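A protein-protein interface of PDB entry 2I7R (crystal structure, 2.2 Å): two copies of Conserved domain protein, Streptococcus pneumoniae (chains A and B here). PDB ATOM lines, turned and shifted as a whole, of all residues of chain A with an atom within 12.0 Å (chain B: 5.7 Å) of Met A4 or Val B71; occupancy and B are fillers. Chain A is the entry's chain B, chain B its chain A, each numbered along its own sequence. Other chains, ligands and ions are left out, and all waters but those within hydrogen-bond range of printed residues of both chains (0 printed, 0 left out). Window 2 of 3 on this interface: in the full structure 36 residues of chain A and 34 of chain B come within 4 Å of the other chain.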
ATOM      1  N   MET A   4      -0.646 -14.226  20.684  1.00  0.00           N
ATOM      2  CA  MET A   4       0.549 -13.733  21.447  1.00  0.00           C
ATOM      3  C   MET A   4       0.304 -12.466  22.271  1.00  0.00           C
ATOM      4  O   MET A   4      -0.318 -11.524  21.797  1.00  0.00           O
ATOM      5  CB  MET A   4       1.715 -13.451  20.502  1.00  0.00           C
ATOM      6  CG  MET A   4       2.586 -14.643  20.118  1.00  0.00           C
ATOM      7  SD  MET A   4       4.038 -14.014  18.924  1.00  0.00           S
ATOM      8  CE  MET A   4       2.926 -12.819  17.850  1.00  0.00           C
ATOM      9  N   ASN A   5       0.849 -12.423  23.488  1.00  0.00           N
ATOM     10  CA  ASN A   5       0.690 -11.246  24.336  1.00  0.00           C
ATOM     11  C   ASN A   5       1.928 -10.923  25.164  1.00  0.00           C
ATOM     12  O   ASN A   5       2.293 -11.667  26.078  1.00  0.00           O
ATOM     13  CB  ASN A   5      -0.561 -11.344  25.233  1.00  0.00           C
ATOM     14  CG  ASN A   5      -0.888 -10.004  25.958  1.00  0.00           C
ATOM     15  OD1 ASN A   5      -0.617  -8.896  25.433  1.00  0.00           O
ATOM     16  ND2 ASN A   5      -1.487 -10.110  27.175  1.00  0.00           N
ATOM     17  N   LEU A   6       2.585  -9.829  24.806  1.00  0.00           N
ATOM     18  CA  LEU A   6       3.722  -9.359  25.573  1.00  0.00           C
ATOM     19  C   LEU A   6       3.230  -8.700  26.921  1.00  0.00           C
ATOM     20  O   LEU A   6       2.720  -7.605  26.911  1.00  0.00           O
ATOM     21  CB  LEU A   6       4.609  -8.445  24.685  1.00  0.00           C
ATOM     22  CG  LEU A   6       5.756  -7.632  25.296  1.00  0.00           C
ATOM     23  CD1 LEU A   6       6.607  -8.527  26.041  1.00  0.00           C
ATOM     24  CD2 LEU A   6       6.564  -6.866  24.256  1.00  0.00           C
ATOM     25  N   ASN A   7       3.398  -9.396  28.048  1.00  0.00           N
ATOM     26  CA  ASN A   7       2.843  -8.967  29.349  1.00  0.00           C
ATOM     27  C   ASN A   7       3.767  -9.051  30.586  1.00  0.00           C
ATOM     28  O   ASN A   7       3.361  -8.777  31.716  1.00  0.00           O
ATOM     29  CB  ASN A   7       1.484  -9.640  29.627  1.00  0.00           C
ATOM     30  CG  ASN A   7       1.585 -11.141  29.842  1.00  0.00           C
ATOM     31  OD1 ASN A   7       2.673 -11.740  29.803  1.00  0.00           O
ATOM     32  ND2 ASN A   7       0.428 -11.771  30.083  1.00  0.00           N
ATOM     33  N   GLN A   8       5.011  -9.446  30.392  1.00  0.00           N
ATOM     34  CA  GLN A   8       5.942  -9.410  31.524  1.00  0.00           C
ATOM     35  C   GLN A   8       7.330  -9.058  31.011  1.00  0.00           C
ATOM     36  O   GLN A   8       7.797  -9.621  30.018  1.00  0.00           O
ATOM     37  CB  GLN A   8       5.948 -10.737  32.291  1.00  0.00           C
ATOM     38  CG  GLN A   8       6.931 -10.796  33.454  1.00  0.00           C
ATOM     39  CD  GLN A   8       6.927 -12.137  34.154  1.00  0.00           C
ATOM     40  OE1 GLN A   8       5.896 -12.809  34.204  1.00  0.00           O
ATOM     41  NE2 GLN A   8       8.075 -12.545  34.686  1.00  0.00           N
ATOM     42  N   SER A  45      -1.896  -3.635  33.044  1.00  0.00           N
ATOM     43  CA  SER A  45      -2.157  -4.977  32.527  1.00  0.00           C
ATOM     44  C   SER A  45      -0.845  -5.692  32.139  1.00  0.00           C
ATOM     45  O   SER A  45      -0.839  -6.707  31.394  1.00  0.00           O
ATOM     46  CB  SER A  45      -3.071  -4.863  31.290  1.00  0.00           C
ATOM     47  OG  SER A  45      -2.430  -4.068  30.271  1.00  0.00           O
ATOM     48  N   HIS A  46       0.271  -5.153  32.607  1.00  0.00           N
ATOM     49  CA  HIS A  46       1.558  -5.727  32.304  1.00  0.00           C
ATOM     50  C   HIS A  46       2.445  -5.734  33.549  1.00  0.00           C
ATOM     51  O   HIS A  46       2.313  -4.886  34.430  1.00  0.00           O
ATOM     52  CB  HIS A  46       2.152  -4.995  31.109  1.00  0.00           C
ATOM     53  CG  HIS A  46       1.198  -4.895  29.952  1.00  0.00           C
ATOM     54  ND1 HIS A  46       0.248  -3.895  29.847  1.00  0.00           N
ATOM     55  CD2 HIS A  46       1.016  -5.691  28.870  1.00  0.00           C
ATOM     56  CE1 HIS A  46      -0.446  -4.059  28.730  1.00  0.00           C
ATOM     57  NE2 HIS A  46      -0.001  -5.143  28.120  1.00  0.00           N
ATOM     58  N   LEU B  27       9.162 -14.039  15.965  1.00  0.00           N
ATOM     59  CA  LEU B  27       7.817 -13.765  16.414  1.00  0.00           C
ATOM     60  C   LEU B  27       6.793 -14.303  15.420  1.00  0.00           C
ATOM     61  O   LEU B  27       5.598 -14.420  15.737  1.00  0.00           O
ATOM     62  CB  LEU B  27       7.620 -12.262  16.571  1.00  0.00           C
ATOM     63  CG  LEU B  27       8.328 -11.546  17.728  1.00  0.00           C
ATOM     64  CD1 LEU B  27       8.198 -10.028  17.547  1.00  0.00           C
ATOM     65  CD2 LEU B  27       7.782 -12.055  19.094  1.00  0.00           C
ATOM     66  N   LYS B  29       5.747 -12.771  12.886  1.00  0.00           N
ATOM     67  CA  LYS B  29       4.886 -11.698  12.366  1.00  0.00           C
ATOM     68  C   LYS B  29       5.747 -10.553  11.920  1.00  0.00           C
ATOM     69  O   LYS B  29       6.845 -10.334  12.473  1.00  0.00           O
ATOM     70  CB  LYS B  29       3.828 -11.224  13.384  1.00  0.00           C
ATOM     71  CG  LYS B  29       4.342 -10.375  14.502  1.00  0.00           C
ATOM     72  CD  LYS B  29       3.243 -10.140  15.531  1.00  0.00           C
ATOM     73  CE  LYS B  29       2.193  -9.170  15.037  1.00  0.00           C
ATOM     74  NZ  LYS B  29       0.979  -9.276  15.907  1.00  0.00           N
ATOM     75  N   THR B  42       3.511  -4.849  17.126  1.00  0.00           N
ATOM     76  CA  THR B  42       2.422  -5.005  18.087  1.00  0.00           C
ATOM     77  C   THR B  42       2.392  -6.490  18.488  1.00  0.00           C
ATOM     78  O   THR B  42       2.440  -7.386  17.634  1.00  0.00           O
ATOM     79  CB  THR B  42       1.094  -4.492  17.481  1.00  0.00           C
ATOM     80  OG1 THR B  42       1.256  -3.099  17.131  1.00  0.00           O
ATOM     81  CG2 THR B  42      -0.078  -4.634  18.463  1.00  0.00           C
ATOM     82  N   ILE B  43       2.408  -6.746  19.788  1.00  0.00           N
ATOM     83  CA  ILE B  43       2.335  -8.098  20.297  1.00  0.00           C
ATOM     84  C   ILE B  43       1.216  -8.175  21.315  1.00  0.00           C
ATOM     85  O   ILE B  43       1.442  -8.007  22.529  1.00  0.00           O
ATOM     86  CB  ILE B  43       3.656  -8.593  20.944  1.00  0.00           C
ATOM     87  CG1 ILE B  43       4.899  -8.267  20.075  1.00  0.00           C
ATOM     88  CG2 ILE B  43       3.541 -10.085  21.210  1.00  0.00           C
ATOM     89  CD1 ILE B  43       6.274  -8.422  20.792  1.00  0.00           C
ATOM     90  N   GLY B  44       0.014  -8.440  20.812  1.00  0.00           N
ATOM     91  CA  GLY B  44      -1.193  -8.454  21.630  1.00  0.00           C
ATOM     92  C   GLY B  44      -1.496  -7.028  22.048  1.00  0.00           C
ATOM     93  O   GLY B  44      -1.741  -6.177  21.215  1.00  0.00           O
ATOM     94  N   SER B  45      -1.388  -6.781  23.348  1.00  0.00           N
ATOM     95  CA  SER B  45      -1.746  -5.520  24.000  1.00  0.00           C
ATOM     96  C   SER B  45      -0.538  -4.649  24.273  1.00  0.00           C
ATOM     97  O   SER B  45      -0.637  -3.676  25.040  1.00  0.00           O
ATOM     98  CB  SER B  45      -2.347  -5.844  25.371  1.00  0.00           C
ATOM     99  OG  SER B  45      -1.332  -6.455  26.201  1.00  0.00           O
ATOM    100  N   ILE B  69       6.315 -13.529  26.465  1.00  0.00           N
ATOM    101  CA  ILE B  69       5.162 -13.461  25.587  1.00  0.00           C
ATOM    102  C   ILE B  69       4.230 -14.620  25.889  1.00  0.00           C
ATOM    103  O   ILE B  69       4.601 -15.809  25.715  1.00  0.00           O
ATOM    104  CB  ILE B  69       5.565 -13.457  24.090  1.00  0.00           C
ATOM    105  CG1 ILE B  69       6.523 -12.285  23.820  1.00  0.00           C
ATOM    106  CG2 ILE B  69       4.286 -13.393  23.152  1.00  0.00           C
ATOM    107  CD1 ILE B  69       7.264 -12.355  22.504  1.00  0.00           C
ATOM    108  N   GLU B  70       3.037 -14.293  26.382  1.00  0.00           N
ATOM    109  CA  GLU B  70       2.060 -15.332  26.643  1.00  0.00           C
ATOM    110  C   GLU B  70       1.425 -15.847  25.332  1.00  0.00           C
ATOM    111  O   GLU B  70       0.949 -15.073  24.498  1.00  0.00           O
ATOM    112  CB  GLU B  70       0.990 -14.870  27.623  1.00  0.00           C
ATOM    113  CG  GLU B  70       0.311 -16.060  28.318  1.00  0.00           C
ATOM    114  CD  GLU B  70      -0.588 -15.653  29.471  1.00  0.00           C
ATOM    115  OE1 GLU B  70      -0.795 -14.431  29.686  1.00  0.00           O
ATOM    116  OE2 GLU B  70      -1.088 -16.575  30.154  1.00  0.00           O
ATOM    117  N   VAL B  71       1.468 -17.162  25.151  1.00  0.00           N
ATOM    118  CA  VAL B  71       0.996 -17.792  23.916  1.00  0.00           C
ATOM    119  C   VAL B  71       0.019 -18.937  24.253  1.00  0.00           C
ATOM    120  O   VAL B  71      -0.003 -19.401  25.398  1.00  0.00           O
ATOM    121  CB  VAL B  71       2.176 -18.365  23.075  1.00  0.00           C
ATOM    122  CG1 VAL B  71       3.058 -17.257  22.568  1.00  0.00           C
ATOM    123  CG2 VAL B  71       2.985 -19.410  23.884  1.00  0.00           C
ATOM    124  N   GLU B  72      -0.754 -19.385  23.262  1.00  0.00           N
ATOM    125  CA  GLU B  72      -1.653 -20.526  23.457  1.00  0.00           C
ATOM    126  C   GLU B  72      -0.937 -21.881  23.402  1.00  0.00           C
ATOM    127  O   GLU B  72      -1.283 -22.796  24.143  1.00  0.00           O
ATOM    128  CB  GLU B  72      -2.821 -20.486  22.452  1.00  0.00           C
ATOM    129  CG  GLU B  72      -3.900 -19.378  22.744  1.00  0.00           C
ATOM    130  CD  GLU B  72      -5.208 -19.901  23.417  1.00  0.00           C
ATOM    131  OE1 GLU B  72      -5.416 -21.140  23.532  1.00  0.00           O
ATOM    132  OE2 GLU B  72      -6.053 -19.055  23.816  1.00  0.00           O
ATOM    133  N   ASP B  73       0.073 -21.999  22.541  1.00  0.00           N
ATOM    134  CA  ASP B  73       0.761 -23.280  22.346  1.00  0.00           C
ATOM    135  C   ASP B  73       2.275 -23.088  22.318  1.00  0.00           C
ATOM    136  O   ASP B  73       2.827 -22.649  21.302  1.00  0.00           O
ATOM    137  CB  ASP B  73       0.254 -23.966  21.049  1.00  0.00           C
ATOM    138  CG  ASP B  73       0.622 -25.459  20.962  1.00  0.00           C
ATOM    139  OD1 ASP B  73       1.596 -25.910  21.583  1.00  0.00           O
ATOM    140  OD2 ASP B  73      -0.074 -26.193  20.228  1.00  0.00           O
ATOM    141  N   VAL B  74       2.930 -23.444  23.431  1.00  0.00           N
ATOM    142  CA  VAL B  74       4.362 -23.293  23.601  1.00  0.00           C
ATOM    143  C   VAL B  74       5.153 -24.258  22.725  1.00  0.00           C
ATOM    144  O   VAL B  74       6.171 -23.890  22.109  1.00  0.00           O
ATOM    145  CB  VAL B  74       4.779 -23.425  25.095  1.00  0.00           C
ATOM    146  CG1 VAL B  74       6.296 -23.394  25.275  1.00  0.00           C
ATOM    147  CG2 VAL B  74       4.133 -22.317  25.913  1.00  0.00           C
ATOM    148  N   ASN B  77       5.254 -23.292  19.008  1.00  0.00           N
ATOM    149  CA  ASN B  77       6.303 -22.288  18.831  1.00  0.00           C
ATOM    150  C   ASN B  77       7.678 -22.918  18.842  1.00  0.00           C
ATOM    151  O   ASN B  77       8.533 -22.579  18.024  1.00  0.00           O
ATOM    152  CB  ASN B  77       6.213 -21.184  19.894  1.00  0.00           C
ATOM    153  CG  ASN B  77       5.149 -20.161  19.563  1.00  0.00           C
ATOM    154  OD1 ASN B  77       5.362 -19.283  18.734  1.00  0.00           O
ATOM    155  ND2 ASN B  77       3.984 -20.299  20.182  1.00  0.00           N
ATOM    156  N   PHE B 114       8.503 -17.580  25.421  1.00  0.00           N
ATOM    157  CA  PHE B 114       7.143 -17.918  25.016  1.00  0.00           C
ATOM    158  C   PHE B 114       6.558 -18.860  26.091  1.00  0.00           C
ATOM    159  O   PHE B 114       7.064 -19.962  26.290  1.00  0.00           O
ATOM    160  CB  PHE B 114       7.148 -18.568  23.628  1.00  0.00           C
ATOM    161  CG  PHE B 114       7.724 -17.680  22.544  1.00  0.00           C
ATOM    162  CD1 PHE B 114       6.899 -16.833  21.815  1.00  0.00           C
ATOM    163  CD2 PHE B 114       9.089 -17.683  22.269  1.00  0.00           C
ATOM    164  CE1 PHE B 114       7.424 -16.017  20.798  1.00  0.00           C
ATOM    165  CE2 PHE B 114       9.633 -16.871  21.253  1.00  0.00           C
ATOM    166  CZ  PHE B 114       8.808 -16.032  20.522  1.00  0.00           C
ATOM    167  N   TYR B 115       5.512 -18.409  26.787  1.00  0.00           N
ATOM    168  CA  TYR B 115       5.008 -19.136  27.945  1.00  0.00           C
ATOM    169  C   TYR B 115       3.467 -19.210  27.989  1.00  0.00           C
ATOM    170  O   TYR B 115       2.789 -18.455  27.319  1.00  0.00           O
ATOM    171  CB  TYR B 115       5.572 -18.543  29.272  1.00  0.00           C
ATOM    172  CG  TYR B 115       4.842 -17.292  29.755  1.00  0.00           C
ATOM    173  CD1 TYR B 115       3.968 -17.337  30.840  1.00  0.00           C
ATOM    174  CD2 TYR B 115       5.014 -16.074  29.096  1.00  0.00           C
ATOM    175  CE1 TYR B 115       3.289 -16.181  31.263  1.00  0.00           C
ATOM    176  CE2 TYR B 115       4.370 -14.937  29.509  1.00  0.00           C
ATOM    177  CZ  TYR B 115       3.507 -14.991  30.592  1.00  0.00           C
ATOM    178  OH  TYR B 115       2.862 -13.837  30.950  1.00  0.00           O
ATOM    179  N   ARG B 116       2.954 -20.155  28.772  1.00  0.00           N
ATOM    180  CA  ARG B 116       1.523 -20.236  29.084  1.00  0.00           C
ATOM    181  C   ARG B 116       1.316 -20.722  30.502  1.00  0.00           C
ATOM    182  O   ARG B 116       2.153 -21.385  31.061  1.00  0.00           O
ATOM    183  CB  ARG B 116       0.714 -21.095  28.067  1.00  0.00           C
ATOM    184  CG  ARG B 116       1.332 -22.401  27.690  1.00  0.00           C
ATOM    185  CD  ARG B 116       0.310 -23.351  26.938  1.00  0.00           C
ATOM    186  NE  ARG B 116      -0.638 -23.816  27.910  1.00  0.00           N
ATOM    187  CZ  ARG B 116      -0.409 -24.777  28.809  1.00  0.00           C
ATOM    188  NH1 ARG B 116       0.711 -25.482  28.812  1.00  0.00           N
ATOM    189  NH2 ARG B 116      -1.345 -25.039  29.712  1.00  0.00           N
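The backbone carbonyl oxygen (O) of Ile B43 is in hydrogen-bond range of the backbone NH (N) of Leu A6, at 3.1 Å.
N of Gly B44 sits close to O of Met A4, at 3.3 Å.
OD1 of Asn A5 sits at hydrogen-bond distance from OG of Ser B45, at 2.7 Å.
OG of Ser B45 sits at hydrogen-bond distance from NE2 of His A46, 2.7 Å away.
The backbone NH of Glu B70 lies within hydrogen-bond range of the backbone carbonyl oxygen of Asn A5.
The side-chain carboxylate of Glu B70 lies within hydrogen-bond range of the side-chain amide nitrogen of Asn A7 (3.0 Å).
The side-chain hydroxyl (OH) of Tyr B115 sits close to the side-chain amide nitrogen (ND2) of Asn A7 (3.3 Å).
The side-chain sulfur of Met A4 lies close to the backbone carbonyl oxygen of Leu B27, 3.6 Å away.
The side-chain amino group (NZ) of Lys B29 is in hydrogen-bond range of the backbone carbonyl oxygen (O) of Thr B42.
The backbone carbonyl oxygen of Ile B69 is in hydrogen-bond range of the backbone NH of Tyr B115, at 3.0 Å.
N of Val B71 is in hydrogen-bond range of O of Tyr B115 (2.8 Å).
The side-chain hydroxyl of Ser A45 lies close to a ring nitrogen (ND1) of His A46 (2.7 Å).
Among the printed residues, pairs that only touch across the chains: Met A4 with Glu B70, Asn A5 with Ile B69, Met A4 with Lys B29, Met A4 with Val B71, Asn A5 with Ile B43, Met A4 with Ile B69, Met A4 with Ile B43 and Asn A5 with Gly B44.
Met A4 touches seven residues of chain B.
Of chain A, only Met A4 comes within 4 Å of Val B71.
Leu B27 touches just one residue of chain A: Met A4.
Printed residues of chain A within 4 Å of Lys B29: Met A4.
Of chain A, only Met A4, Asn A5 and Leu A6 come within 4 Å of Ile B43.
Of chain A, only Met A4 and Asn A5 come within 4 Å of Gly B44.
Glu B70 touches just these residues of chain A: Met A4, Asn A5 and Asn A7.
No residue of chain A comes within 4 Å of Phe B114.
Of chain A, only Asn A7 (2.4 Å) comes within 4 Å of Tyr B115.
Of the printed residues of chain A, Ser B45 touches Asn A5 (2.7 Å) and His A46 (2.7 Å).
Printed residues of chain B within 4 Å of Asn A7: Glu B70 (3.0 Å) and Tyr B115 (2.4 Å).
Printed residues of chain B within 4 Å of His A46: Ser B45.
Of the printed residues of chain B, Leu A6 touches Ile B43 (3.1 Å).
Of the printed residues of chain B, Asn A5 touches Ile B43 (3.7 Å), Gly B44 (3.9 Å), Ser B45 (2.7 Å), Ile B69 (3.4 Å) and Glu B70 (2.7 Å).
Hydrophobic or aromatic side chains of chain B within 4 Å of the printed part of chain A: Ile B43, Ile B69, Val B71 and Tyr B115.
Of the 7 printed residues of chain A, 5 touch a printed residue of chain B.
Hydrophobic or aromatic side chains of chain A within 4 Å of the printed part of chain B: Met A4, Leu A6 and His A46.
Along chain A the printed residues that touch a printed residue of chain B span positions 4 to 46.
Among the printed residues, no Asp or Glu carboxylate lies within 4 Å of a Lys or Arg side-chain nitrogen of the other chain.
Position printed for both chains: 45.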
